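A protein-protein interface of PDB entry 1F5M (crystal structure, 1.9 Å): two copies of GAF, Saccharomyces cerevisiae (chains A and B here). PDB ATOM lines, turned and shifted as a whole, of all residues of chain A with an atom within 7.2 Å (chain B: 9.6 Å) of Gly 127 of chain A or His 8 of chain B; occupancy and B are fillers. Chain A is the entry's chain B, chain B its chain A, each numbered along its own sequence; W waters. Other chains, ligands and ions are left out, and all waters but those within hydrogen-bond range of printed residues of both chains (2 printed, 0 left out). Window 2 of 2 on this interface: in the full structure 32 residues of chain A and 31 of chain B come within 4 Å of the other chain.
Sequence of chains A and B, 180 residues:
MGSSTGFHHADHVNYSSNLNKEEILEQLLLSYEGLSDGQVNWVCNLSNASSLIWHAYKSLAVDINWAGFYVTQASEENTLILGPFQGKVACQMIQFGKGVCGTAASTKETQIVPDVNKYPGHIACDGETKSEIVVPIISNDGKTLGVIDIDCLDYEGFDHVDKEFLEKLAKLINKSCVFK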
ATOM      1  N   ASN A  65     -11.426  26.772  15.829  1.00  0.00           N
ATOM      2  CA  ASN A  65     -11.472  25.538  16.596  1.00  0.00           C
ATOM      3  C   ASN A  65     -10.149  24.788  16.506  1.00  0.00           C
ATOM      4  O   ASN A  65      -9.977  23.762  17.150  1.00  0.00           O
ATOM      5  CB  ASN A  65     -12.625  24.600  16.176  1.00  0.00           C
ATOM      6  CG  ASN A  65     -12.722  24.365  14.673  1.00  0.00           C
ATOM      7  OD1 ASN A  65     -12.805  25.299  13.888  1.00  0.00           O
ATOM      8  ND2 ASN A  65     -12.774  23.099  14.278  1.00  0.00           N
ATOM      9  N   VAL A  89      -8.469  17.062  19.384  1.00  0.00           N
ATOM     10  CA  VAL A  89      -7.667  15.963  18.816  1.00  0.00           C
ATOM     11  C   VAL A  89      -7.788  15.951  17.259  1.00  0.00           C
ATOM     12  O   VAL A  89      -8.857  16.180  16.694  1.00  0.00           O
ATOM     13  CB  VAL A  89      -8.136  14.631  19.488  1.00  0.00           C
ATOM     14  CG1 VAL A  89      -7.661  13.413  18.726  1.00  0.00           C
ATOM     15  CG2 VAL A  89      -7.557  14.592  20.950  1.00  0.00           C
ATOM     16  N   VAL A 116     -14.775  24.157   3.341  1.00  0.00           N
ATOM     17  CA  VAL A 116     -14.009  22.947   3.356  1.00  0.00           C
ATOM     18  C   VAL A 116     -14.716  21.737   2.676  1.00  0.00           C
ATOM     19  O   VAL A 116     -14.079  20.866   2.038  1.00  0.00           O
ATOM     20  CB  VAL A 116     -13.646  22.782   4.871  1.00  0.00           C
ATOM     21  CG1 VAL A 116     -14.240  21.605   5.411  1.00  0.00           C
ATOM     22  CG2 VAL A 116     -12.166  22.968   5.075  1.00  0.00           C
ATOM     23  N   ASN A 117     -16.029  21.711   2.760  1.00  0.00           N
ATOM     24  CA  ASN A 117     -16.764  20.643   2.148  1.00  0.00           C
ATOM     25  C   ASN A 117     -16.909  20.821   0.635  1.00  0.00           C
ATOM     26  O   ASN A 117     -17.408  19.914  -0.051  1.00  0.00           O
ATOM     27  CB  ASN A 117     -18.124  20.514   2.831  1.00  0.00           C
ATOM     28  CG  ASN A 117     -17.977  20.097   4.306  1.00  0.00           C
ATOM     29  OD1 ASN A 117     -17.228  19.165   4.626  1.00  0.00           O
ATOM     30  ND2 ASN A 117     -18.686  20.777   5.191  1.00  0.00           N
ATOM     31  N   HIS A 122     -10.919  16.872   0.912  1.00  0.00           N
ATOM     32  CA  HIS A 122     -10.787  17.419   2.261  1.00  0.00           C
ATOM     33  C   HIS A 122     -10.635  16.271   3.276  1.00  0.00           C
ATOM     34  O   HIS A 122     -11.300  15.258   3.171  1.00  0.00           O
ATOM     35  CB  HIS A 122     -12.045  18.245   2.573  1.00  0.00           C
ATOM     36  CG  HIS A 122     -12.153  18.706   3.996  1.00  0.00           C
ATOM     37  ND1 HIS A 122     -11.113  19.307   4.676  1.00  0.00           N
ATOM     38  CD2 HIS A 122     -13.204  18.700   4.853  1.00  0.00           C
ATOM     39  CE1 HIS A 122     -11.517  19.647   5.887  1.00  0.00           C
ATOM     40  NE2 HIS A 122     -12.781  19.289   6.021  1.00  0.00           N
ATOM     41  N   ILE A 123      -9.762  16.443   4.262  1.00  0.00           N
ATOM     42  CA  ILE A 123      -9.531  15.420   5.301  1.00  0.00           C
ATOM     43  C   ILE A 123      -9.937  16.143   6.558  1.00  0.00           C
ATOM     44  O   ILE A 123      -9.208  17.027   7.011  1.00  0.00           O
ATOM     45  CB  ILE A 123      -8.002  15.013   5.353  1.00  0.00           C
ATOM     46  CG1 ILE A 123      -7.634  14.376   4.015  1.00  0.00           C
ATOM     47  CG2 ILE A 123      -7.733  14.092   6.552  1.00  0.00           C
ATOM     48  CD1 ILE A 123      -6.168  14.035   3.842  1.00  0.00           C
ATOM     49  N   ALA A 124     -11.145  15.850   7.055  1.00  0.00           N
ATOM     50  CA  ALA A 124     -11.656  16.486   8.249  1.00  0.00           C
ATOM     51  C   ALA A 124     -11.175  15.800   9.534  1.00  0.00           C
ATOM     52  O   ALA A 124     -11.416  14.599   9.730  1.00  0.00           O
ATOM     53  CB  ALA A 124     -13.195  16.481   8.221  1.00  0.00           C
ATOM     54  N   CYS A 125     -10.504  16.550  10.398  1.00  0.00           N
ATOM     55  CA  CYS A 125     -10.076  16.007  11.713  1.00  0.00           C
ATOM     56  C   CYS A 125     -11.238  16.380  12.671  1.00  0.00           C
ATOM     57  O   CYS A 125     -11.585  15.651  13.608  1.00  0.00           O
ATOM     58  CB  CYS A 125      -8.737  16.627  12.150  1.00  0.00           C
ATOM     59  SG  CYS A 125      -7.424  16.329  10.909  1.00  0.00           S
ATOM     60  N   ASP A 126     -11.844  17.524  12.418  1.00  0.00           N
ATOM     61  CA  ASP A 126     -12.985  17.999  13.216  1.00  0.00           C
ATOM     62  C   ASP A 126     -14.148  18.110  12.236  1.00  0.00           C
ATOM     63  O   ASP A 126     -14.088  18.877  11.255  1.00  0.00           O
ATOM     64  CB  ASP A 126     -12.686  19.372  13.853  1.00  0.00           C
ATOM     65  CG  ASP A 126     -13.786  19.814  14.869  1.00  0.00           C
ATOM     66  OD1 ASP A 126     -14.990  19.493  14.665  1.00  0.00           O
ATOM     67  OD2 ASP A 126     -13.448  20.501  15.874  1.00  0.00           O
ATOM     68  N   GLY A 127     -15.201  17.335  12.479  1.00  0.00           N
ATOM     69  CA  GLY A 127     -16.344  17.395  11.592  1.00  0.00           C
ATOM     70  C   GLY A 127     -17.014  18.756  11.577  1.00  0.00           C
ATOM     71  O   GLY A 127     -17.817  19.013  10.673  1.00  0.00           O
ATOM     72  N   GLU A 128     -16.709  19.641  12.540  1.00  0.00           N
ATOM     73  CA  GLU A 128     -17.376  20.962  12.527  1.00  0.00           C
ATOM     74  C   GLU A 128     -16.618  22.047  11.813  1.00  0.00           C
ATOM     75  O   GLU A 128     -17.085  23.185  11.746  1.00  0.00           O
ATOM     76  CB  GLU A 128     -17.639  21.459  13.938  1.00  0.00           C
ATOM     77  CG  GLU A 128     -18.927  20.950  14.487  1.00  0.00           C
ATOM     78  CD  GLU A 128     -18.687  20.306  15.821  1.00  0.00           C
ATOM     79  OE1 GLU A 128     -18.907  20.958  16.879  1.00  0.00           O
ATOM     80  OE2 GLU A 128     -18.239  19.127  15.787  1.00  0.00           O
ATOM     81  N   THR A 129     -15.437  21.716  11.290  1.00  0.00           N
ATOM     82  CA  THR A 129     -14.668  22.715  10.629  1.00  0.00           C
ATOM     83  C   THR A 129     -15.411  23.107   9.343  1.00  0.00           C
ATOM     84  O   THR A 129     -15.855  22.232   8.601  1.00  0.00           O
ATOM     85  CB  THR A 129     -13.238  22.167  10.300  1.00  0.00           C
ATOM     86  OG1 THR A 129     -12.505  21.954  11.522  1.00  0.00           O
ATOM     87  CG2 THR A 129     -12.468  23.181   9.437  1.00  0.00           C
ATOM     88  N   LYS A 130     -15.563  24.408   9.090  1.00  0.00           N
ATOM     89  CA  LYS A 130     -16.220  24.867   7.859  1.00  0.00           C
ATOM     90  C   LYS A 130     -15.281  25.613   6.941  1.00  0.00           C
ATOM     91  O   LYS A 130     -15.492  25.626   5.736  1.00  0.00           O
ATOM     92  CB  LYS A 130     -17.430  25.767   8.175  1.00  0.00           C
ATOM     93  CG  LYS A 130     -18.704  24.973   8.411  1.00  0.00           C
ATOM     94  CD  LYS A 130     -19.824  25.883   8.943  1.00  0.00           C
ATOM     95  CE  LYS A 130     -21.047  24.957   9.180  1.00  0.00           C
ATOM     96  NZ  LYS A 130     -22.185  25.703   9.718  1.00  0.00           N
ATOM     97  N   LEU A 153     -14.918  27.535  12.638  1.00  0.00           N
ATOM     98  CA  LEU A 153     -16.267  26.965  12.710  1.00  0.00           C
ATOM     99  C   LEU A 153     -17.260  27.578  11.746  1.00  0.00           C
ATOM    100  O   LEU A 153     -18.325  27.013  11.543  1.00  0.00           O
ATOM    101  CB  LEU A 153     -16.832  27.090  14.120  1.00  0.00           C
ATOM    102  CG  LEU A 153     -16.061  26.232  15.139  1.00  0.00           C
ATOM    103  CD1 LEU A 153     -16.617  26.489  16.527  1.00  0.00           C
ATOM    104  CD2 LEU A 153     -16.191  24.782  14.801  1.00  0.00           C
ATOM    105  N   SER B   4     -17.984   4.065   6.305  1.00  0.00           N
ATOM    106  CA  SER B   4     -17.750   5.319   7.114  1.00  0.00           C
ATOM    107  C   SER B   4     -18.275   5.214   8.537  1.00  0.00           C
ATOM    108  O   SER B   4     -19.490   5.087   8.741  1.00  0.00           O
ATOM    109  CB  SER B   4     -18.414   6.539   6.460  1.00  0.00           C
ATOM    110  OG  SER B   4     -17.981   7.753   7.093  1.00  0.00           O
ATOM    111  N   THR B   5     -17.381   5.324   9.524  1.00  0.00           N
ATOM    112  CA  THR B   5     -17.804   5.224  10.915  1.00  0.00           C
ATOM    113  C   THR B   5     -18.754   6.347  11.331  1.00  0.00           C
ATOM    114  O   THR B   5     -19.569   6.159  12.221  1.00  0.00           O
ATOM    115  CB  THR B   5     -16.622   5.284  11.896  1.00  0.00           C
ATOM    116  OG1 THR B   5     -16.023   6.592  11.845  1.00  0.00           O
ATOM    117  CG2 THR B   5     -15.577   4.217  11.567  1.00  0.00           C
ATOM    118  N   GLY B   6     -18.642   7.507  10.688  1.00  0.00           N
ATOM    119  CA  GLY B   6     -19.453   8.662  11.058  1.00  0.00           C
ATOM    120  C   GLY B   6     -18.720   9.504  12.114  1.00  0.00           C
ATOM    121  O   GLY B   6     -19.174  10.608  12.459  1.00  0.00           O
ATOM    122  N   PHE B   7     -17.610   8.983  12.649  1.00  0.00           N
ATOM    123  CA  PHE B   7     -16.799   9.695  13.666  1.00  0.00           C
ATOM    124  C   PHE B   7     -15.652  10.542  13.066  1.00  0.00           C
ATOM    125  O   PHE B   7     -15.253  10.370  11.915  1.00  0.00           O
ATOM    126  CB  PHE B   7     -16.158   8.705  14.657  1.00  0.00           C
ATOM    127  CG  PHE B   7     -17.132   7.992  15.544  1.00  0.00           C
ATOM    128  CD1 PHE B   7     -17.317   6.604  15.429  1.00  0.00           C
ATOM    129  CD2 PHE B   7     -17.872   8.689  16.501  1.00  0.00           C
ATOM    130  CE1 PHE B   7     -18.225   5.923  16.252  1.00  0.00           C
ATOM    131  CE2 PHE B   7     -18.800   8.015  17.336  1.00  0.00           C
ATOM    132  CZ  PHE B   7     -18.977   6.633  17.208  1.00  0.00           C
ATOM    133  N   HIS B   8     -15.116  11.464  13.859  1.00  0.00           N
ATOM    134  CA  HIS B   8     -13.995  12.272  13.410  1.00  0.00           C
ATOM    135  C   HIS B   8     -13.056  12.264  14.621  1.00  0.00           C
ATOM    136  O   HIS B   8     -13.530  12.043  15.745  1.00  0.00           O
ATOM    137  CB  HIS B   8     -14.420  13.711  13.099  1.00  0.00           C
ATOM    138  CG  HIS B   8     -15.213  13.859  11.836  1.00  0.00           C
ATOM    139  ND1 HIS B   8     -16.599  13.824  11.813  1.00  0.00           N
ATOM    140  CD2 HIS B   8     -14.821  14.061  10.559  1.00  0.00           C
ATOM    141  CE1 HIS B   8     -17.019  13.993  10.571  1.00  0.00           C
ATOM    142  NE2 HIS B   8     -15.957  14.137   9.787  1.00  0.00           N
ATOM    143  N   HIS B   9     -11.754  12.460  14.395  1.00  0.00           N
ATOM    144  CA  HIS B   9     -10.785  12.500  15.512  1.00  0.00           C
ATOM    145  C   HIS B   9     -11.254  13.375  16.657  1.00  0.00           C
ATOM    146  O   HIS B   9     -11.108  13.008  17.834  1.00  0.00           O
ATOM    147  CB  HIS B   9      -9.432  13.052  15.061  1.00  0.00           C
ATOM    148  CG  HIS B   9      -8.646  12.102  14.210  1.00  0.00           C
ATOM    149  ND1 HIS B   9      -9.054  11.726  12.946  1.00  0.00           N
ATOM    150  CD2 HIS B   9      -7.501  11.425  14.452  1.00  0.00           C
ATOM    151  CE1 HIS B   9      -8.191  10.857  12.448  1.00  0.00           C
ATOM    152  NE2 HIS B   9      -7.240  10.656  13.342  1.00  0.00           N
ATOM    153  N   ALA B  10     -11.777  14.552  16.312  1.00  0.00           N
ATOM    154  CA  ALA B  10     -12.241  15.521  17.318  1.00  0.00           C
ATOM    155  C   ALA B  10     -13.230  14.963  18.349  1.00  0.00           C
ATOM    156  O   ALA B  10     -13.251  15.391  19.507  1.00  0.00           O
ATOM    157  CB  ALA B  10     -12.856  16.729  16.623  1.00  0.00           C
ATOM    158  N   ASP B  11     -14.039  14.000  17.924  1.00  0.00           N
ATOM    159  CA  ASP B  11     -15.087  13.397  18.754  1.00  0.00           C
ATOM    160  C   ASP B  11     -14.584  12.780  20.077  1.00  0.00           C
ATOM    161  O   ASP B  11     -15.367  12.585  20.994  1.00  0.00           O
ATOM    162  CB  ASP B  11     -15.826  12.325  17.942  1.00  0.00           C
ATOM    163  CG  ASP B  11     -16.602  12.915  16.767  1.00  0.00           C
ATOM    164  OD1 ASP B  11     -16.866  12.190  15.783  1.00  0.00           O
ATOM    165  OD2 ASP B  11     -16.954  14.118  16.828  1.00  0.00           O
ATOM    166  N   HIS B  12     -13.303  12.456  20.150  1.00  0.00           N
ATOM    167  CA  HIS B  12     -12.727  11.910  21.378  1.00  0.00           C
ATOM    168  C   HIS B  12     -12.888  12.887  22.544  1.00  0.00           C
ATOM    169  O   HIS B  12     -12.834  12.477  23.705  1.00  0.00           O
ATOM    170  CB  HIS B  12     -11.230  11.631  21.187  1.00  0.00           C
ATOM    171  CG  HIS B  12     -10.930  10.349  20.467  1.00  0.00           C
ATOM    172  ND1 HIS B  12     -10.910   9.123  21.103  1.00  0.00           N
ATOM    173  CD2 HIS B  12     -10.658  10.101  19.160  1.00  0.00           C
ATOM    174  CE1 HIS B  12     -10.635   8.177  20.213  1.00  0.00           C
ATOM    175  NE2 HIS B  12     -10.484   8.744  19.027  1.00  0.00           N
ATOM    176  N   VAL B  13     -13.073  14.176  22.270  1.00  0.00           N
ATOM    177  CA  VAL B  13     -13.193  15.099  23.385  1.00  0.00           C
ATOM    178  C   VAL B  13     -14.586  15.553  23.730  1.00  0.00           C
ATOM    179  O   VAL B  13     -14.804  16.691  24.069  1.00  0.00           O
ATOM    180  CB  VAL B  13     -12.251  16.346  23.270  1.00  0.00           C
ATOM    181  CG1 VAL B  13     -10.796  15.890  23.338  1.00  0.00           C
ATOM    182  CG2 VAL B  13     -12.525  17.147  21.967  1.00  0.00           C
ATOM    183  N   ASN B  14     -15.521  14.624  23.652  1.00  0.00           N
ATOM    184  CA  ASN B  14     -16.909  14.848  24.041  1.00  0.00           C
ATOM    185  C   ASN B  14     -17.175  14.128  25.331  1.00  0.00           C
ATOM    186  O   ASN B  14     -16.956  12.910  25.449  1.00  0.00           O
ATOM    187  CB  ASN B  14     -17.847  14.324  22.987  1.00  0.00           C
ATOM    188  CG  ASN B  14     -18.070  15.330  21.934  1.00  0.00           C
ATOM    189  OD1 ASN B  14     -17.122  15.772  21.272  1.00  0.00           O
ATOM    190  ND2 ASN B  14     -19.327  15.753  21.782  1.00  0.00           N
ATOM    191  N   SER B  31      -8.995   6.515  24.751  1.00  0.00           N
ATOM    192  CA  SER B  31      -8.832   7.345  23.527  1.00  0.00           C
ATOM    193  C   SER B  31      -7.337   7.484  23.211  1.00  0.00           C
ATOM    194  O   SER B  31      -6.962   7.402  22.052  1.00  0.00           O
ATOM    195  CB  SER B  31      -9.398   8.752  23.711  1.00  0.00           C
ATOM    196  OG  SER B  31     -10.803   8.743  23.799  1.00  0.00           O
ATOM    197  N   LEU B  35      -5.662   6.550  19.723  1.00  0.00           N
ATOM    198  CA  LEU B  35      -4.979   7.536  18.895  1.00  0.00           C
ATOM    199  C   LEU B  35      -3.494   7.333  18.708  1.00  0.00           C
ATOM    200  O   LEU B  35      -2.981   7.734  17.687  1.00  0.00           O
ATOM    201  CB  LEU B  35      -5.213   8.948  19.423  1.00  0.00           C
ATOM    202  CG  LEU B  35      -6.695   9.359  19.349  1.00  0.00           C
ATOM    203  CD1 LEU B  35      -7.050  10.306  20.472  1.00  0.00           C
ATOM    204  CD2 LEU B  35      -6.948   9.997  17.961  1.00  0.00           C
HETATM  205  O   HOH W   1     -16.345  16.253  14.940  1.00  0.00           O
HETATM  206  O   HOH W   2     -11.413  12.580  11.359  1.00  0.00           O
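N of Ala 10 of chain B lies within hydrogen-bond range of O of Val 89 of chain A (3.4 Å).
The backbone carbonyl oxygen of Cys 125 of chain A is in hydrogen-bond range of the backbone NH of His 9 of chain B (3.3 Å).
The backbone NH (N) of Ala 10 of chain B lies within hydrogen-bond range of the backbone carbonyl oxygen (O) of Cys 125 of chain A (2.9 Å).
O of Asp 126 of chain A sits at hydrogen-bond distance from OG1 of Thr 129 of chain A (3.5 Å).
OD2 of Asp 126 of chain A lies within hydrogen-bond range of ND2 of Asn 65 of chain A (3.1 Å).
N of His 8 of chain B lies within hydrogen-bond range of OD1 of Asp 11 of chain B (2.7 Å).
The backbone NH of Glu 128 of chain A is in hydrogen-bond range of the side-chain carboxylate of Asp 126 of chain A.
O of Val 89 of chain A touches CB of His 9 of chain B (3.6 Å).
Val 89 of chain A touches Leu 35 of chain B.
Ala 124 of chain A touches His 8 of chain B.
CB of His 8 of chain B touches O of Cys 125 of chain A (3.5 Å).
CB of Ala 10 of chain B touches CA of Asp 126 of chain A, at 3.6 Å.
Gly 127 of chain A touches His 8 of chain B (N to CG, 3.5 Å).
Of chain B, only His 8 (3.5 Å) comes within 4 Å of Gly 127 of chain A.
His 8 of chain B touches three residues of chain A.
Printed residues of chain A within 4 Å of Ala 10 of chain B: Val 89, Cys 125 and Asp 126.
Printed residues of chain B within 4 Å of Cys 125 of chain A: His 8 (3.5 Å), His 9 (3.3 Å) and Ala 10 (2.9 Å).
Printed residues of chain B within 4 Å of Val 89 of chain A: His 9 (3.6 Å), Ala 10 (3.4 Å) and Leu 35 (3.6 Å).
Asn 65 of chain A touches none of the printed residues of chain B.
Thr 129 of chain A touches none of the printed residues of chain B.
The nearest residue of chain A that does not touch His 8 of chain B is Asp 126 of chain A (4.4 Å).
The nearest printed residue of chain A that does not touch Ala 10 of chain B is Gly 127 of chain A (4.8 Å).
Of the 13 printed residues of chain B, 4 touch a printed residue of chain A.
Printed residues of chain B that touch a printed residue of chain A: His 8, His 9, Ala 10 and Leu 35.
Hydrophobic or aromatic side chains of chain B within 4 Å of the printed part of chain A: His 8, His 9, Ala 10 and Leu 35.
Of the 14 printed residues of chain A, 5 touch a printed residue of chain B.
No position is printed for both chains.
Of the 9 pairs that touch across the chains among the printed residues, none has its exchanged pair printed and touching as well.
Water W2 lies within hydrogen-bond range of O of Ala 124 of chain A (2.6 Å) and ND1 of His 9 of chain B (3.0 Å).
Water W1 bridges the side-chain carboxylate of Asp 11 of chain B (2.9 Å) and the backbone NH of Gly 127 of chain A (2.9 Å).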
